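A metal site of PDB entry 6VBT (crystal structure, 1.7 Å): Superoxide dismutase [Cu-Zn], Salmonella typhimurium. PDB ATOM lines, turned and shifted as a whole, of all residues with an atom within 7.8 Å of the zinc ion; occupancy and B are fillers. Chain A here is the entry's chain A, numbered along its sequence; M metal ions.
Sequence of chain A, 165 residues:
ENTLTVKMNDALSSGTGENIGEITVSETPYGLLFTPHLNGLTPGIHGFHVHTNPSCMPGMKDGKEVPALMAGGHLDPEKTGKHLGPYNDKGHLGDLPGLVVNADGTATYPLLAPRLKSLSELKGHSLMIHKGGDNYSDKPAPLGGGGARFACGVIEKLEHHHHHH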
ATOM      1  N   PHE A  48       9.550  -8.602  -3.549  1.00  0.00           N
ATOM      2  CA  PHE A  48      10.157  -7.870  -2.434  1.00  0.00           C
ATOM      3  C   PHE A  48      10.993  -8.883  -1.657  1.00  0.00           C
ATOM      4  O   PHE A  48      10.444  -9.819  -1.075  1.00  0.00           O
ATOM      5  CB  PHE A  48       9.061  -7.227  -1.590  1.00  0.00           C
ATOM      6  CG  PHE A  48       9.563  -6.420  -0.427  1.00  0.00           C
ATOM      7  CD1 PHE A  48      10.616  -5.540  -0.562  1.00  0.00           C
ATOM      8  CD2 PHE A  48       8.925  -6.520   0.802  1.00  0.00           C
ATOM      9  CE1 PHE A  48      11.043  -4.799   0.517  1.00  0.00           C
ATOM     10  CE2 PHE A  48       9.349  -5.774   1.873  1.00  0.00           C
ATOM     11  CZ  PHE A  48      10.414  -4.906   1.738  1.00  0.00           C
ATOM     12  N   HIS A  49      12.308  -8.717  -1.670  1.00  0.00           N
ATOM     13  CA  HIS A  49      13.183  -9.728  -1.091  1.00  0.00           C
ATOM     14  C   HIS A  49      14.406  -9.101  -0.436  1.00  0.00           C
ATOM     15  O   HIS A  49      14.865  -8.027  -0.840  1.00  0.00           O
ATOM     16  CB  HIS A  49      13.680 -10.731  -2.154  1.00  0.00           C
ATOM     17  CG  HIS A  49      12.660 -11.048  -3.205  1.00  0.00           C
ATOM     18  ND1 HIS A  49      12.754 -10.576  -4.493  1.00  0.00           N
ATOM     19  CD2 HIS A  49      11.517 -11.774  -3.152  1.00  0.00           C
ATOM     20  CE1 HIS A  49      11.715 -10.999  -5.194  1.00  0.00           C
ATOM     21  NE2 HIS A  49      10.947 -11.725  -4.401  1.00  0.00           N
ATOM     22  N   VAL A  50      14.934  -9.786   0.571  1.00  0.00           N
ATOM     23  CA  VAL A  50      16.249  -9.461   1.107  1.00  0.00           C
ATOM     24  C   VAL A  50      17.292 -10.120   0.212  1.00  0.00           C
ATOM     25  O   VAL A  50      17.216 -11.327  -0.053  1.00  0.00           O
ATOM     26  CB  VAL A  50      16.382  -9.948   2.557  1.00  0.00           C
ATOM     27  CG1 VAL A  50      17.679  -9.439   3.174  1.00  0.00           C
ATOM     28  CG2 VAL A  50      15.192  -9.517   3.384  1.00  0.00           C
ATOM     29  N   HIS A  51      18.263  -9.344  -0.236  1.00  0.00           N
ATOM     30  CA  HIS A  51      19.372  -9.854  -1.030  1.00  0.00           C
ATOM     31  C   HIS A  51      20.633  -9.951  -0.161  1.00  0.00           C
ATOM     32  O   HIS A  51      20.750  -9.306   0.882  1.00  0.00           O
ATOM     33  CB  HIS A  51      19.622  -8.966  -2.251  1.00  0.00           C
ATOM     34  CG  HIS A  51      18.606  -9.162  -3.329  1.00  0.00           C
ATOM     35  ND1 HIS A  51      18.945  -9.554  -4.615  1.00  0.00           N
ATOM     36  CD2 HIS A  51      17.249  -9.042  -3.324  1.00  0.00           C
ATOM     37  CE1 HIS A  51      17.845  -9.670  -5.342  1.00  0.00           C
ATOM     38  NE2 HIS A  51      16.813  -9.358  -4.587  1.00  0.00           N
ATOM     39  N   GLY A  73      22.028 -12.296  -5.040  1.00  0.00           N
ATOM     40  CA  GLY A  73      20.736 -12.923  -5.152  1.00  0.00           C
ATOM     41  C   GLY A  73      19.955 -12.878  -3.855  1.00  0.00           C
ATOM     42  O   GLY A  73      20.310 -12.175  -2.907  1.00  0.00           O
ATOM     43  N   HIS A  74      18.869 -13.645  -3.811  1.00  0.00           N
ATOM     44  CA  HIS A  74      18.019 -13.694  -2.630  1.00  0.00           C
ATOM     45  C   HIS A  74      18.786 -14.296  -1.469  1.00  0.00           C
ATOM     46  O   HIS A  74      19.452 -15.321  -1.603  1.00  0.00           O
ATOM     47  CB  HIS A  74      16.769 -14.525  -2.906  1.00  0.00           C
ATOM     48  CG  HIS A  74      15.843 -13.929  -3.923  1.00  0.00           C
ATOM     49  ND1 HIS A  74      14.577 -14.412  -4.156  1.00  0.00           N
ATOM     50  CD2 HIS A  74      16.013 -12.898  -4.782  1.00  0.00           C
ATOM     51  CE1 HIS A  74      13.998 -13.704  -5.105  1.00  0.00           C
ATOM     52  NE2 HIS A  74      14.849 -12.777  -5.515  1.00  0.00           N
ATOM     53  N   LEU A  75      18.685 -13.645  -0.302  1.00  0.00           N
ATOM     54  CA  LEU A  75      19.357 -14.145   0.883  1.00  0.00           C
ATOM     55  C   LEU A  75      19.004 -15.601   1.128  1.00  0.00           C
ATOM     56  O   LEU A  75      17.821 -15.951   1.274  1.00  0.00           O
ATOM     57  CB  LEU A  75      18.980 -13.289   2.095  1.00  0.00           C
ATOM     58  CG  LEU A  75      19.553 -13.755   3.437  1.00  0.00           C
ATOM     59  CD1 LEU A  75      21.071 -13.745   3.411  1.00  0.00           C
ATOM     60  CD2 LEU A  75      19.015 -12.871   4.543  1.00  0.00           C
ATOM     61  N   ASP A  76      20.020 -16.466   1.176  1.00  0.00           N
ATOM     62  CA  ASP A  76      19.801 -17.911   1.228  1.00  0.00           C
ATOM     63  C   ASP A  76      20.902 -18.588   2.031  1.00  0.00           C
ATOM     64  O   ASP A  76      21.633 -19.427   1.492  1.00  0.00           O
ATOM     65  CB  ASP A  76      19.748 -18.463  -0.201  1.00  0.00           C
ATOM     66  CG  ASP A  76      19.273 -19.906  -0.270  1.00  0.00           C
ATOM     67  OD1 ASP A  76      18.716 -20.426   0.725  1.00  0.00           O
ATOM     68  OD2 ASP A  76      19.447 -20.528  -1.349  1.00  0.00           O
ATOM     69  N   THR A  80      19.385 -23.279  -0.115  1.00  0.00           N
ATOM     70  CA  THR A  80      18.276 -24.043  -0.675  1.00  0.00           C
ATOM     71  C   THR A  80      18.223 -23.947  -2.193  1.00  0.00           C
ATOM     72  O   THR A  80      17.810 -24.899  -2.864  1.00  0.00           O
ATOM     73  CB  THR A  80      16.941 -23.579  -0.079  1.00  0.00           C
ATOM     74  OG1 THR A  80      16.653 -22.249  -0.546  1.00  0.00           O
ATOM     75  CG2 THR A  80      16.991 -23.594   1.440  1.00  0.00           C
ATOM     76  N   GLY A  81      18.615 -22.804  -2.751  1.00  0.00           N
ATOM     77  CA  GLY A  81      18.470 -22.567  -4.174  1.00  0.00           C
ATOM     78  C   GLY A  81      17.046 -22.600  -4.653  1.00  0.00           C
ATOM     79  O   GLY A  81      16.805 -22.831  -5.841  1.00  0.00           O
ATOM     80  N   LYS A  82      16.077 -22.361  -3.757  1.00  0.00           N
ATOM     81  CA  LYS A  82      14.668 -22.467  -4.076  1.00  0.00           C
ATOM     82  C   LYS A  82      13.953 -21.198  -3.629  1.00  0.00           C
ATOM     83  O   LYS A  82      14.140 -20.747  -2.497  1.00  0.00           O
ATOM     84  CB  LYS A  82      14.025 -23.672  -3.398  1.00  0.00           C
ATOM     85  CG  LYS A  82      14.359 -25.024  -4.019  1.00  0.00           C
ATOM     86  CD  LYS A  82      13.832 -26.159  -3.146  1.00  0.00           C
ATOM     87  CE  LYS A  82      14.361 -27.509  -3.595  1.00  0.00           C
ATOM     88  NZ  LYS A  82      13.264 -28.409  -4.045  1.00  0.00           N
ATOM     89  N   HIS A  83      13.140 -20.638  -4.528  1.00  0.00           N
ATOM     90  CA  HIS A  83      12.296 -19.486  -4.199  1.00  0.00           C
ATOM     91  C   HIS A  83      10.903 -20.004  -3.852  1.00  0.00           C
ATOM     92  O   HIS A  83      10.168 -20.461  -4.727  1.00  0.00           O
ATOM     93  CB  HIS A  83      12.239 -18.502  -5.368  1.00  0.00           C
ATOM     94  CG  HIS A  83      11.427 -17.291  -5.078  1.00  0.00           C
ATOM     95  ND1 HIS A  83      11.893 -16.229  -4.337  1.00  0.00           N
ATOM     96  CD2 HIS A  83      10.144 -16.974  -5.401  1.00  0.00           C
ATOM     97  CE1 HIS A  83      10.945 -15.312  -4.220  1.00  0.00           C
ATOM     98  NE2 HIS A  83       9.874 -15.750  -4.857  1.00  0.00           N
ATOM     99  N   LEU A  84      10.549 -19.951  -2.566  1.00  0.00           N
ATOM    100  CA  LEU A  84       9.280 -20.512  -2.108  1.00  0.00           C
ATOM    101  C   LEU A  84       8.478 -19.537  -1.251  1.00  0.00           C
ATOM    102  O   LEU A  84       7.445 -19.919  -0.702  1.00  0.00           O
ATOM    103  CB  LEU A  84       9.531 -21.805  -1.335  1.00  0.00           C
ATOM    104  CG  LEU A  84       9.983 -22.979  -2.213  1.00  0.00           C
ATOM    105  CD1 LEU A  84      10.459 -24.139  -1.348  1.00  0.00           C
ATOM    106  CD2 LEU A  84       8.847 -23.418  -3.120  1.00  0.00           C
ATOM    107  N   GLY A  85       8.924 -18.293  -1.105  1.00  0.00           N
ATOM    108  CA  GLY A  85       8.123 -17.272  -0.479  1.00  0.00           C
ATOM    109  C   GLY A  85       8.280 -17.215   1.017  1.00  0.00           C
ATOM    110  O   GLY A  85       9.047 -17.977   1.628  1.00  0.00           O
ATOM    111  N   GLY A  91      12.740 -22.594   1.317  1.00  0.00           N
ATOM    112  CA  GLY A  91      13.309 -21.714   0.325  1.00  0.00           C
ATOM    113  C   GLY A  91      14.095 -20.567   0.907  1.00  0.00           C
ATOM    114  O   GLY A  91      14.355 -20.535   2.116  1.00  0.00           O
ATOM    115  N   HIS A  92      14.471 -19.620   0.054  1.00  0.00           N
ATOM    116  CA  HIS A  92      15.302 -18.489   0.450  1.00  0.00           C
ATOM    117  C   HIS A  92      14.757 -17.820   1.700  1.00  0.00           C
ATOM    118  O   HIS A  92      13.587 -17.431   1.744  1.00  0.00           O
ATOM    119  CB  HIS A  92      15.347 -17.447  -0.661  1.00  0.00           C
ATOM    120  CG  HIS A  92      15.711 -17.973  -2.014  1.00  0.00           C
ATOM    121  ND1 HIS A  92      15.077 -17.567  -3.159  1.00  0.00           N
ATOM    122  CD2 HIS A  92      16.688 -18.824  -2.397  1.00  0.00           C
ATOM    123  CE1 HIS A  92      15.623 -18.152  -4.200  1.00  0.00           C
ATOM    124  NE2 HIS A  92      16.606 -18.924  -3.764  1.00  0.00           N
ATOM    125  N   LEU A  93      15.629 -17.637   2.702  1.00  0.00           N
ATOM    126  CA  LEU A  93      15.227 -16.910   3.895  1.00  0.00           C
ATOM    127  C   LEU A  93      14.824 -15.479   3.570  1.00  0.00           C
ATOM    128  O   LEU A  93      13.995 -14.893   4.278  1.00  0.00           O
ATOM    129  CB  LEU A  93      16.348 -16.916   4.922  1.00  0.00           C
ATOM    130  CG  LEU A  93      16.011 -16.257   6.269  1.00  0.00           C
ATOM    131  CD1 LEU A  93      14.877 -16.972   6.964  1.00  0.00           C
ATOM    132  CD2 LEU A  93      17.256 -16.219   7.164  1.00  0.00           C
ATOM    133  N   GLY A  94      15.423 -14.890   2.539  1.00  0.00           N
ATOM    134  CA  GLY A  94      15.138 -13.521   2.181  1.00  0.00           C
ATOM    135  C   GLY A  94      13.822 -13.275   1.472  1.00  0.00           C
ATOM    136  O   GLY A  94      13.547 -12.132   1.084  1.00  0.00           O
ATOM    137  N   ASP A  95      13.018 -14.303   1.274  1.00  0.00           N
ATOM    138  CA  ASP A  95      11.750 -14.167   0.554  1.00  0.00           C
ATOM    139  C   ASP A  95      10.739 -13.482   1.465  1.00  0.00           C
ATOM    140  O   ASP A  95      10.286 -14.076   2.449  1.00  0.00           O
ATOM    141  CB  ASP A  95      11.245 -15.525   0.093  1.00  0.00           C
ATOM    142  CG  ASP A  95      12.048 -16.109  -1.046  1.00  0.00           C
ATOM    143  OD1 ASP A  95      12.929 -15.408  -1.602  1.00  0.00           O
ATOM    144  OD2 ASP A  95      11.786 -17.272  -1.385  1.00  0.00           O
ATOM    145  N   LEU A  96      10.372 -12.250   1.142  1.00  0.00           N
ATOM    146  CA  LEU A  96       9.361 -11.493   1.874  1.00  0.00           C
ATOM    147  C   LEU A  96       8.027 -11.547   1.139  1.00  0.00           C
ATOM    148  O   LEU A  96       7.957 -11.942  -0.029  1.00  0.00           O
ATOM    149  CB  LEU A  96       9.823 -10.045   2.050  1.00  0.00           C
ATOM    150  CG  LEU A  96      11.243  -9.820   2.559  1.00  0.00           C
ATOM    151  CD1 LEU A  96      11.570  -8.325   2.656  1.00  0.00           C
ATOM    152  CD2 LEU A  96      11.453 -10.499   3.901  1.00  0.00           C
ATOM    153  N   ARG A 115       9.198 -15.614   9.067  1.00  0.00           N
ATOM    154  CA  ARG A 115      10.407 -16.423   9.160  1.00  0.00           C
ATOM    155  C   ARG A 115      11.599 -15.646   9.721  1.00  0.00           C
ATOM    156  O   ARG A 115      12.569 -16.262  10.169  1.00  0.00           O
ATOM    157  CB  ARG A 115      10.766 -16.999   7.793  1.00  0.00           C
ATOM    158  CG  ARG A 115       9.710 -17.934   7.244  1.00  0.00           C
ATOM    159  CD  ARG A 115       9.983 -18.298   5.816  1.00  0.00           C
ATOM    160  NE  ARG A 115      11.278 -18.954   5.673  1.00  0.00           N
ATOM    161  CZ  ARG A 115      11.979 -19.003   4.539  1.00  0.00           C
ATOM    162  NH1 ARG A 115      11.490 -18.440   3.444  1.00  0.00           N
ATOM    163  NH2 ARG A 115      13.153 -19.624   4.512  1.00  0.00           N
ATOM    164  N   ASP A 134       5.218 -11.625  -7.381  1.00  0.00           N
ATOM    165  CA  ASP A 134       5.827 -12.766  -6.704  1.00  0.00           C
ATOM    166  C   ASP A 134       4.739 -13.797  -6.413  1.00  0.00           C
ATOM    167  O   ASP A 134       3.874 -13.558  -5.556  1.00  0.00           O
ATOM    168  CB  ASP A 134       6.519 -12.352  -5.408  1.00  0.00           C
ATOM    169  CG  ASP A 134       7.505 -13.398  -4.904  1.00  0.00           C
ATOM    170  OD1 ASP A 134       7.471 -14.548  -5.397  1.00  0.00           O
ATOM    171  OD2 ASP A 134       8.316 -13.071  -4.025  1.00  0.00           O
ATOM    172  N   TYR A 136       5.646 -16.714  -5.283  1.00  0.00           N
ATOM    173  CA  TYR A 136       6.284 -17.552  -4.275  1.00  0.00           C
ATOM    174  C   TYR A 136       6.716 -18.899  -4.845  1.00  0.00           C
ATOM    175  O   TYR A 136       6.746 -19.906  -4.122  1.00  0.00           O
ATOM    176  CB  TYR A 136       5.372 -17.736  -3.064  1.00  0.00           C
ATOM    177  CG  TYR A 136       4.873 -16.433  -2.459  1.00  0.00           C
ATOM    178  CD1 TYR A 136       5.622 -15.269  -2.564  1.00  0.00           C
ATOM    179  CD2 TYR A 136       3.665 -16.381  -1.779  1.00  0.00           C
ATOM    180  CE1 TYR A 136       5.178 -14.080  -2.023  1.00  0.00           C
ATOM    181  CE2 TYR A 136       3.212 -15.184  -1.230  1.00  0.00           C
ATOM    182  CZ  TYR A 136       3.963 -14.035  -1.370  1.00  0.00           C
ATOM    183  OH  TYR A 136       3.485 -12.857  -0.847  1.00  0.00           O
ATOM    184  N   SER A 137       7.098 -18.922  -6.123  1.00  0.00           N
ATOM    185  CA  SER A 137       7.505 -20.155  -6.786  1.00  0.00           C
ATOM    186  C   SER A 137       8.537 -19.822  -7.855  1.00  0.00           C
ATOM    187  O   SER A 137       8.658 -18.680  -8.297  1.00  0.00           O
ATOM    188  CB  SER A 137       6.298 -20.874  -7.404  1.00  0.00           C
ATOM    189  OG  SER A 137       6.666 -22.063  -8.063  1.00  0.00           O
ATOM    190  N   ASP A 138       9.281 -20.840  -8.273  1.00  0.00           N
ATOM    191  CA  ASP A 138      10.174 -20.716  -9.403  1.00  0.00           C
ATOM    192  C   ASP A 138       9.501 -21.085 -10.716  1.00  0.00           C
ATOM    193  O   ASP A 138      10.142 -21.019 -11.770  1.00  0.00           O
ATOM    194  CB  ASP A 138      11.414 -21.574  -9.191  1.00  0.00           C
ATOM    195  CG  ASP A 138      12.450 -20.888  -8.305  1.00  0.00           C
ATOM    196  OD1 ASP A 138      12.743 -19.691  -8.547  1.00  0.00           O
ATOM    197  OD2 ASP A 138      12.984 -21.560  -7.379  1.00  0.00           O
ATOM    198  N   LEU A 143      12.235 -17.183  -9.634  1.00  0.00           N
ATOM    199  CA  LEU A 143      12.235 -16.181  -8.566  1.00  0.00           C
ATOM    200  C   LEU A 143      10.895 -15.464  -8.468  1.00  0.00           C
ATOM    201  O   LEU A 143      10.829 -14.258  -8.222  1.00  0.00           O
ATOM    202  CB  LEU A 143      13.373 -15.186  -8.775  1.00  0.00           C
ATOM    203  CG  LEU A 143      14.784 -15.783  -8.878  1.00  0.00           C
ATOM    204  CD1 LEU A 143      15.820 -14.675  -9.005  1.00  0.00           C
ATOM    205  CD2 LEU A 143      15.081 -16.669  -7.694  1.00  0.00           C
ATOM    206  N   GLY A 144       9.816 -16.220  -8.654  1.00  0.00           N
ATOM    207  CA  GLY A 144       8.486 -15.685  -8.447  1.00  0.00           C
ATOM    208  C   GLY A 144       7.962 -14.786  -9.536  1.00  0.00           C
ATOM    209  O   GLY A 144       6.853 -14.244  -9.398  1.00  0.00           O
HETATM  210 ZN    ZN M   1      13.668 -16.049  -3.266  1.00  0.00          ZN
HETATM  211 CU    CU M   2      14.716  -9.748  -5.021  1.00  0.00          CU
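The side-chain carboxylate (OD2) of Asp 95 is in hydrogen-bond range of the backbone NH (N) of Leu 84, at 3.2 Å. OD2 of Asp 95 lies within hydrogen-bond range of N of Gly 85, at 3.1 Å. ND1 of His 49 lies close to NE2 of His 74 (3.2 Å). The backbone carbonyl oxygen (O) of Lys 82 sits at hydrogen-bond distance from the backbone NH (N) of His 92, 2.8 Å away. The backbone NH (N) of His 92 is in hydrogen-bond range of the side-chain hydroxyl (OG1) of Thr 80 (3.5 Å). O of His 92 is in hydrogen-bond range of NH1 of Arg 115 (2.9 Å). A ring nitrogen (NE2) of His 83 sits at hydrogen-bond distance from the side-chain carboxylate (OD1) of Asp 134 (2.7 Å). The backbone NH (N) of His 83 is in hydrogen-bond range of the side-chain carboxylate (OD2) of Asp 138, 3.0 Å away.
Of the 27 residues printed, 4 come within 4 Å of the zinc ion.
The zinc ion is bound by the side-chain carboxylate of Asp 95 (1.9 Å), a ring nitrogen (ND1) of His 74 (2.1 Å), a ring nitrogen (ND1) of His 92 (2.1 Å) and a ring nitrogen (ND1) of His 83 (2.1 Å).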
